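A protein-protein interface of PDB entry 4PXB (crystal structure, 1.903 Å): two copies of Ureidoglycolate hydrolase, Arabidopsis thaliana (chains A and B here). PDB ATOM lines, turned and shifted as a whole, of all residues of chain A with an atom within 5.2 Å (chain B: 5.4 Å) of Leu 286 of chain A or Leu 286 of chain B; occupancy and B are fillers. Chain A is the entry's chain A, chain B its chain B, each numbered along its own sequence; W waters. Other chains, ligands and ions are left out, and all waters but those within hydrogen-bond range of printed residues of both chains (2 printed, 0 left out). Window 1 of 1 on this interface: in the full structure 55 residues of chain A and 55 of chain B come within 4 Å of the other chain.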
ATOM      1  N   ALA A 260       8.132 -30.203 -16.106  1.00  0.00           N
ATOM      2  CA  ALA A 260       7.685 -30.634 -14.780  1.00  0.00           C
ATOM      3  C   ALA A 260       6.415 -29.890 -14.373  1.00  0.00           C
ATOM      4  O   ALA A 260       5.468 -30.496 -13.865  1.00  0.00           O
ATOM      5  CB  ALA A 260       8.784 -30.423 -13.748  1.00  0.00           C
ATOM      6  N   ALA A 261       6.393 -28.577 -14.608  1.00  0.00           N
ATOM      7  CA  ALA A 261       5.218 -27.760 -14.300  1.00  0.00           C
ATOM      8  C   ALA A 261       3.981 -28.302 -15.006  1.00  0.00           C
ATOM      9  O   ALA A 261       2.919 -28.440 -14.400  1.00  0.00           O
ATOM     10  CB  ALA A 261       5.452 -26.303 -14.701  1.00  0.00           C
ATOM     11  N   ALA A 264       2.806 -31.643 -13.513  1.00  0.00           N
ATOM     12  CA  ALA A 264       2.114 -31.495 -12.230  1.00  0.00           C
ATOM     13  C   ALA A 264       0.649 -31.101 -12.416  1.00  0.00           C
ATOM     14  O   ALA A 264      -0.243 -31.624 -11.737  1.00  0.00           O
ATOM     15  CB  ALA A 264       2.830 -30.481 -11.337  1.00  0.00           C
ATOM     16  N   VAL A 283       1.614 -33.692  -6.366  1.00  0.00           N
ATOM     17  CA  VAL A 283       3.044 -33.566  -6.600  1.00  0.00           C
ATOM     18  C   VAL A 283       3.645 -32.890  -5.368  1.00  0.00           C
ATOM     19  O   VAL A 283       3.598 -31.661  -5.224  1.00  0.00           O
ATOM     20  CB  VAL A 283       3.344 -32.768  -7.884  1.00  0.00           C
ATOM     21  CG1 VAL A 283       4.847 -32.574  -8.054  1.00  0.00           C
ATOM     22  CG2 VAL A 283       2.777 -33.495  -9.105  1.00  0.00           C
ATOM     23  N   GLY A 284       4.193 -33.704  -4.468  1.00  0.00           N
ATOM     24  CA  GLY A 284       4.728 -33.205  -3.218  1.00  0.00           C
ATOM     25  C   GLY A 284       6.174 -32.774  -3.331  1.00  0.00           C
ATOM     26  O   GLY A 284       6.661 -31.985  -2.516  1.00  0.00           O
ATOM     27  N   ILE A 285       6.859 -33.294  -4.349  1.00  0.00           N
ATOM     28  CA  ILE A 285       8.265 -33.001  -4.558  1.00  0.00           C
ATOM     29  C   ILE A 285       8.461 -32.612  -6.009  1.00  0.00           C
ATOM     30  O   ILE A 285       8.047 -33.346  -6.912  1.00  0.00           O
ATOM     31  CB  ILE A 285       9.146 -34.229  -4.243  1.00  0.00           C
ATOM     32  CG1 ILE A 285       9.311 -34.403  -2.734  1.00  0.00           C
ATOM     33  CG2 ILE A 285      10.520 -34.098  -4.905  1.00  0.00           C
ATOM     34  CD1 ILE A 285       9.998 -35.707  -2.336  1.00  0.00           C
ATOM     35  N   LEU A 286       9.063 -31.446  -6.228  1.00  0.00           N
ATOM     36  CA  LEU A 286       9.440 -31.016  -7.566  1.00  0.00           C
ATOM     37  C   LEU A 286      10.763 -30.264  -7.445  1.00  0.00           C
ATOM     38  O   LEU A 286      10.799 -29.144  -6.925  1.00  0.00           O
ATOM     39  CB  LEU A 286       8.349 -30.129  -8.176  1.00  0.00           C
ATOM     40  CG  LEU A 286       8.338 -29.918  -9.700  1.00  0.00           C
ATOM     41  CD1 LEU A 286       7.019 -29.289 -10.128  1.00  0.00           C
ATOM     42  CD2 LEU A 286       9.507 -29.052 -10.167  1.00  0.00           C
ATOM     43  N   GLU A 287      11.849 -30.882  -7.912  1.00  0.00           N
ATOM     44  CA  GLU A 287      13.163 -30.247  -7.812  1.00  0.00           C
ATOM     45  C   GLU A 287      13.771 -29.958  -9.173  1.00  0.00           C
ATOM     46  O   GLU A 287      13.634 -30.759 -10.116  1.00  0.00           O
ATOM     47  CB  GLU A 287      14.141 -31.090  -6.983  1.00  0.00           C
ATOM     48  CG  GLU A 287      14.235 -32.532  -7.411  1.00  0.00           C
ATOM     49  CD  GLU A 287      15.624 -33.137  -7.212  1.00  0.00           C
ATOM     50  OE1 GLU A 287      16.164 -33.710  -8.187  1.00  0.00           O
ATOM     51  OE2 GLU A 287      16.178 -33.028  -6.092  1.00  0.00           O
ATOM     52  N   LEU A 288      14.456 -28.819  -9.261  1.00  0.00           N
ATOM     53  CA  LEU A 288      15.120 -28.416 -10.495  1.00  0.00           C
ATOM     54  C   LEU A 288      16.634 -28.543 -10.333  1.00  0.00           C
ATOM     55  O   LEU A 288      17.180 -28.282  -9.252  1.00  0.00           O
ATOM     56  CB  LEU A 288      14.752 -26.979 -10.865  1.00  0.00           C
ATOM     57  CG  LEU A 288      13.258 -26.657 -11.027  1.00  0.00           C
ATOM     58  CD1 LEU A 288      13.052 -25.206 -11.468  1.00  0.00           C
ATOM     59  CD2 LEU A 288      12.593 -27.626 -12.007  1.00  0.00           C
ATOM     60  N   SER A 300      14.647 -32.010 -14.267  1.00  0.00           N
ATOM     61  CA  SER A 300      13.633 -31.818 -13.239  1.00  0.00           C
ATOM     62  C   SER A 300      13.174 -33.171 -12.741  1.00  0.00           C
ATOM     63  O   SER A 300      13.192 -34.169 -13.476  1.00  0.00           O
ATOM     64  CB  SER A 300      12.457 -31.010 -13.780  1.00  0.00           C
ATOM     65  OG  SER A 300      11.877 -31.665 -14.902  1.00  0.00           O
ATOM     66  N   HIS A 301      12.753 -33.204 -11.481  1.00  0.00           N
ATOM     67  CA  HIS A 301      12.444 -34.451 -10.815  1.00  0.00           C
ATOM     68  C   HIS A 301      11.126 -34.253 -10.072  1.00  0.00           C
ATOM     69  O   HIS A 301      10.962 -33.275  -9.335  1.00  0.00           O
ATOM     70  CB  HIS A 301      13.619 -34.798  -9.887  1.00  0.00           C
ATOM     71  CG  HIS A 301      13.333 -35.840  -8.853  1.00  0.00           C
ATOM     72  ND1 HIS A 301      13.542 -37.191  -9.069  1.00  0.00           N
ATOM     73  CD2 HIS A 301      12.923 -35.734  -7.565  1.00  0.00           C
ATOM     74  CE1 HIS A 301      13.245 -37.864  -7.975  1.00  0.00           C
ATOM     75  NE2 HIS A 301      12.870 -37.001  -7.043  1.00  0.00           N
ATOM     76  N   LEU A 302      10.166 -35.136 -10.330  1.00  0.00           N
ATOM     77  CA  LEU A 302       8.871 -35.073  -9.650  1.00  0.00           C
ATOM     78  C   LEU A 302       8.647 -36.360  -8.890  1.00  0.00           C
ATOM     79  O   LEU A 302       8.990 -37.442  -9.382  1.00  0.00           O
ATOM     80  CB  LEU A 302       7.726 -34.924 -10.657  1.00  0.00           C
ATOM     81  CG  LEU A 302       7.679 -33.732 -11.605  1.00  0.00           C
ATOM     82  CD1 LEU A 302       8.415 -34.057 -12.910  1.00  0.00           C
ATOM     83  CD2 LEU A 302       6.220 -33.343 -11.872  1.00  0.00           C
ATOM     84  N   GLU A 303       8.072 -36.260  -7.692  1.00  0.00           N
ATOM     85  CA  GLU A 303       7.600 -37.455  -7.018  1.00  0.00           C
ATOM     86  C   GLU A 303       6.106 -37.292  -6.801  1.00  0.00           C
ATOM     87  O   GLU A 303       5.650 -36.295  -6.218  1.00  0.00           O
ATOM     88  CB  GLU A 303       8.380 -37.711  -5.726  1.00  0.00           C
ATOM     89  CG  GLU A 303       9.878 -37.796  -5.994  1.00  0.00           C
ATOM     90  CD  GLU A 303      10.679 -38.431  -4.871  1.00  0.00           C
ATOM     91  OE1 GLU A 303      10.104 -39.197  -4.061  1.00  0.00           O
ATOM     92  OE2 GLU A 303      11.904 -38.164  -4.809  1.00  0.00           O
ATOM     93  N   ALA B 260       2.729 -22.388  -8.133  1.00  0.00           N
ATOM     94  CA  ALA B 260       4.069 -22.169  -8.685  1.00  0.00           C
ATOM     95  C   ALA B 260       4.189 -22.685 -10.118  1.00  0.00           C
ATOM     96  O   ALA B 260       4.768 -22.019 -10.974  1.00  0.00           O
ATOM     97  CB  ALA B 260       5.133 -22.822  -7.799  1.00  0.00           C
ATOM     98  N   ALA B 261       3.650 -23.878 -10.370  1.00  0.00           N
ATOM     99  CA  ALA B 261       3.650 -24.445 -11.708  1.00  0.00           C
ATOM    100  C   ALA B 261       2.959 -23.497 -12.686  1.00  0.00           C
ATOM    101  O   ALA B 261       3.455 -23.234 -13.787  1.00  0.00           O
ATOM    102  CB  ALA B 261       2.954 -25.813 -11.700  1.00  0.00           C
ATOM    103  N   ALA B 264       5.144 -20.379 -13.307  1.00  0.00           N
ATOM    104  CA  ALA B 264       6.292 -20.684 -14.159  1.00  0.00           C
ATOM    105  C   ALA B 264       5.864 -20.676 -15.618  1.00  0.00           C
ATOM    106  O   ALA B 264       6.566 -20.134 -16.484  1.00  0.00           O
ATOM    107  CB  ALA B 264       6.911 -22.038 -13.788  1.00  0.00           C
ATOM    108  N   VAL B 283      12.537 -19.601 -15.017  1.00  0.00           N
ATOM    109  CA  VAL B 283      12.413 -19.977 -13.617  1.00  0.00           C
ATOM    110  C   VAL B 283      13.505 -21.001 -13.343  1.00  0.00           C
ATOM    111  O   VAL B 283      13.363 -22.183 -13.675  1.00  0.00           O
ATOM    112  CB  VAL B 283      11.035 -20.582 -13.321  1.00  0.00           C
ATOM    113  CG1 VAL B 283      10.948 -21.012 -11.859  1.00  0.00           C
ATOM    114  CG2 VAL B 283       9.939 -19.567 -13.642  1.00  0.00           C
ATOM    115  N   GLY B 284      14.614 -20.547 -12.768  1.00  0.00           N
ATOM    116  CA  GLY B 284      15.738 -21.434 -12.515  1.00  0.00           C
ATOM    117  C   GLY B 284      15.662 -22.080 -11.148  1.00  0.00           C
ATOM    118  O   GLY B 284      16.352 -23.061 -10.869  1.00  0.00           O
ATOM    119  N   ILE B 285      14.814 -21.529 -10.287  1.00  0.00           N
ATOM    120  CA  ILE B 285      14.637 -22.080  -8.954  1.00  0.00           C
ATOM    121  C   ILE B 285      13.150 -22.184  -8.663  1.00  0.00           C
ATOM    122  O   ILE B 285      12.396 -21.214  -8.828  1.00  0.00           O
ATOM    123  CB  ILE B 285      15.330 -21.208  -7.884  1.00  0.00           C
ATOM    124  CG1 ILE B 285      16.854 -21.369  -7.981  1.00  0.00           C
ATOM    125  CG2 ILE B 285      14.833 -21.571  -6.465  1.00  0.00           C
ATOM    126  CD1 ILE B 285      17.624 -20.511  -6.998  1.00  0.00           C
ATOM    127  N   LEU B 286      12.729 -23.383  -8.291  1.00  0.00           N
ATOM    128  CA  LEU B 286      11.364 -23.619  -7.842  1.00  0.00           C
ATOM    129  C   LEU B 286      11.440 -24.651  -6.719  1.00  0.00           C
ATOM    130  O   LEU B 286      11.739 -25.819  -6.971  1.00  0.00           O
ATOM    131  CB  LEU B 286      10.506 -24.119  -9.007  1.00  0.00           C
ATOM    132  CG  LEU B 286       8.981 -24.077  -8.837  1.00  0.00           C
ATOM    133  CD1 LEU B 286       8.298 -24.252 -10.188  1.00  0.00           C
ATOM    134  CD2 LEU B 286       8.491 -25.148  -7.871  1.00  0.00           C
ATOM    135  N   GLU B 287      11.176 -24.212  -5.489  1.00  0.00           N
ATOM    136  CA  GLU B 287      11.265 -25.077  -4.313  1.00  0.00           C
ATOM    137  C   GLU B 287       9.901 -25.268  -3.663  1.00  0.00           C
ATOM    138  O   GLU B 287       9.175 -24.297  -3.449  1.00  0.00           O
ATOM    139  CB  GLU B 287      12.164 -24.447  -3.261  1.00  0.00           C
ATOM    140  CG  GLU B 287      13.647 -24.643  -3.439  1.00  0.00           C
ATOM    141  CD  GLU B 287      14.428 -23.803  -2.445  1.00  0.00           C
ATOM    142  OE1 GLU B 287      13.971 -23.687  -1.280  1.00  0.00           O
ATOM    143  OE2 GLU B 287      15.481 -23.241  -2.832  1.00  0.00           O
ATOM    144  N   LEU B 288       9.571 -26.508  -3.319  1.00  0.00           N
ATOM    145  CA  LEU B 288       8.346 -26.786  -2.575  1.00  0.00           C
ATOM    146  C   LEU B 288       8.640 -27.098  -1.111  1.00  0.00           C
ATOM    147  O   LEU B 288       9.635 -27.753  -0.798  1.00  0.00           O
ATOM    148  CB  LEU B 288       7.620 -27.976  -3.186  1.00  0.00           C
ATOM    149  CG  LEU B 288       7.328 -27.885  -4.674  1.00  0.00           C
ATOM    150  CD1 LEU B 288       6.549 -29.113  -5.115  1.00  0.00           C
ATOM    151  CD2 LEU B 288       6.554 -26.601  -4.983  1.00  0.00           C
ATOM    152  N   SER B 300       5.524 -22.442  -1.704  1.00  0.00           N
ATOM    153  CA  SER B 300       6.380 -22.632  -2.862  1.00  0.00           C
ATOM    154  C   SER B 300       7.199 -21.369  -3.066  1.00  0.00           C
ATOM    155  O   SER B 300       6.754 -20.275  -2.727  1.00  0.00           O
ATOM    156  CB  SER B 300       5.568 -22.980  -4.111  1.00  0.00           C
ATOM    157  OG  SER B 300       4.643 -21.950  -4.440  1.00  0.00           O
ATOM    158  N   HIS B 301       8.397 -21.535  -3.612  1.00  0.00           N
ATOM    159  CA  HIS B 301       9.331 -20.430  -3.765  1.00  0.00           C
ATOM    160  C   HIS B 301       9.877 -20.480  -5.192  1.00  0.00           C
ATOM    161  O   HIS B 301      10.306 -21.538  -5.661  1.00  0.00           O
ATOM    162  CB  HIS B 301      10.416 -20.586  -2.683  1.00  0.00           C
ATOM    163  CG  HIS B 301      11.590 -19.663  -2.828  1.00  0.00           C
ATOM    164  ND1 HIS B 301      11.621 -18.405  -2.275  1.00  0.00           N
ATOM    165  CD2 HIS B 301      12.792 -19.845  -3.429  1.00  0.00           C
ATOM    166  CE1 HIS B 301      12.791 -17.833  -2.550  1.00  0.00           C
ATOM    167  NE2 HIS B 301      13.513 -18.687  -3.243  1.00  0.00           N
ATOM    168  N   LEU B 302       9.770 -19.363  -5.911  1.00  0.00           N
ATOM    169  CA  LEU B 302      10.282 -19.273  -7.272  1.00  0.00           C
ATOM    170  C   LEU B 302      11.272 -18.134  -7.337  1.00  0.00           C
ATOM    171  O   LEU B 302      11.057 -17.090  -6.726  1.00  0.00           O
ATOM    172  CB  LEU B 302       9.169 -18.972  -8.287  1.00  0.00           C
ATOM    173  CG  LEU B 302       8.022 -19.964  -8.497  1.00  0.00           C
ATOM    174  CD1 LEU B 302       6.875 -19.659  -7.521  1.00  0.00           C
ATOM    175  CD2 LEU B 302       7.541 -19.928  -9.951  1.00  0.00           C
ATOM    176  N   GLU B 303      12.354 -18.326  -8.084  1.00  0.00           N
ATOM    177  CA  GLU B 303      13.239 -17.214  -8.397  1.00  0.00           C
ATOM    178  C   GLU B 303      13.321 -17.113  -9.908  1.00  0.00           C
ATOM    179  O   GLU B 303      13.613 -18.100 -10.598  1.00  0.00           O
ATOM    180  CB  GLU B 303      14.606 -17.404  -7.739  1.00  0.00           C
ATOM    181  CG  GLU B 303      14.467 -17.622  -6.227  1.00  0.00           C
ATOM    182  CD  GLU B 303      15.771 -17.468  -5.465  1.00  0.00           C
ATOM    183  OE1 GLU B 303      16.722 -16.849  -5.999  1.00  0.00           O
ATOM    184  OE2 GLU B 303      15.836 -17.963  -4.318  1.00  0.00           O
HETATM  185  O   HOH W   1      11.630 -28.308  -4.279  1.00  0.00           O
HETATM  186  O   HOH W   2      14.208 -27.352  -6.845  1.00  0.00           O
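N of Gly 284 of chain A is in hydrogen-bond range of O of Glu 303 of chain A (3.4 Å).
The backbone carbonyl oxygen of Glu 303 of chain B sits at hydrogen-bond distance from the backbone NH of Gly 284 of chain B, 3.4 Å away.
Ala 261 of chain B touches its own counterpart, Ala 261 of chain A.
Gly 284 of chain A touches Leu 288 of chain B, and with the chains exchanged Leu 288 of chain A touches Gly 284 of chain B.
Leu 286 of chain B touches its own counterpart, Leu 286 of chain A.
Leu 286 of chain A touches Leu 288 of chain B, and with the chains exchanged Leu 288 of chain A touches Leu 286 of chain B.
Of the 8 pairs that touch across the chains among the printed residues, 8 have their exchanged pair printed and touching as well.
Water W2 lies within hydrogen-bond range of N of Leu 288 of chain A (2.8 Å) and O of Leu 286 of chain B (2.9 Å).
Water W1 lies within hydrogen-bond range of O of Leu 286 of chain A and N of Leu 288 of chain B.
Printed residues of chain B that touch a printed residue of chain A: Ala 261, Val 283, Gly 284, Leu 286 and Leu 288.
Among the printed residues, no Asp or Glu carboxylate lies within 4 Å of a Lys or Arg side-chain nitrogen of the other chain.
O of Leu 286 of chain A sits close to O of Leu 286 of chain B (3.5 Å).
Ala 261 of chain A touches Ala 261 of chain B.
Val 283 of chain A touches Leu 288 of chain B.
Leu 288 of chain B touches Gly 284 of chain A (CD1 to O, 3.9 Å).
N of Leu 286 of chain A touches CD1 of Leu 288 of chain B, at 3.6 Å.
O of Val 283 of chain B touches CD1 of Leu 288 of chain A, at 3.8 Å.
CD1 of Leu 288 of chain A touches O of Gly 284 of chain B, 3.98 Å away.
CD1 of Leu 288 of chain A touches N of Leu 286 of chain B (3.7 Å).
Leu 286 of chain A touches just these residues of chain B: Leu 286 (3.5 Å) and Leu 288 (3.6 Å).
Of the printed residues of chain A, Leu 286 of chain B touches Leu 286 (3.5 Å) and Leu 288 (3.7 Å).
Printed residues of chain A within 4 Å of Gly 284 of chain B: Leu 288 (3.98 Å).
Of the printed residues of chain B, Ala 261 of chain A touches Ala 261.
Ser 300 of chain A touches none of the printed residues of chain B.
His 301 of chain B touches none of the printed residues of chain A.
The nearest printed residue of chain B that does not touch Ala 261 of chain A is Ala 264 of chain B (4.6 Å).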
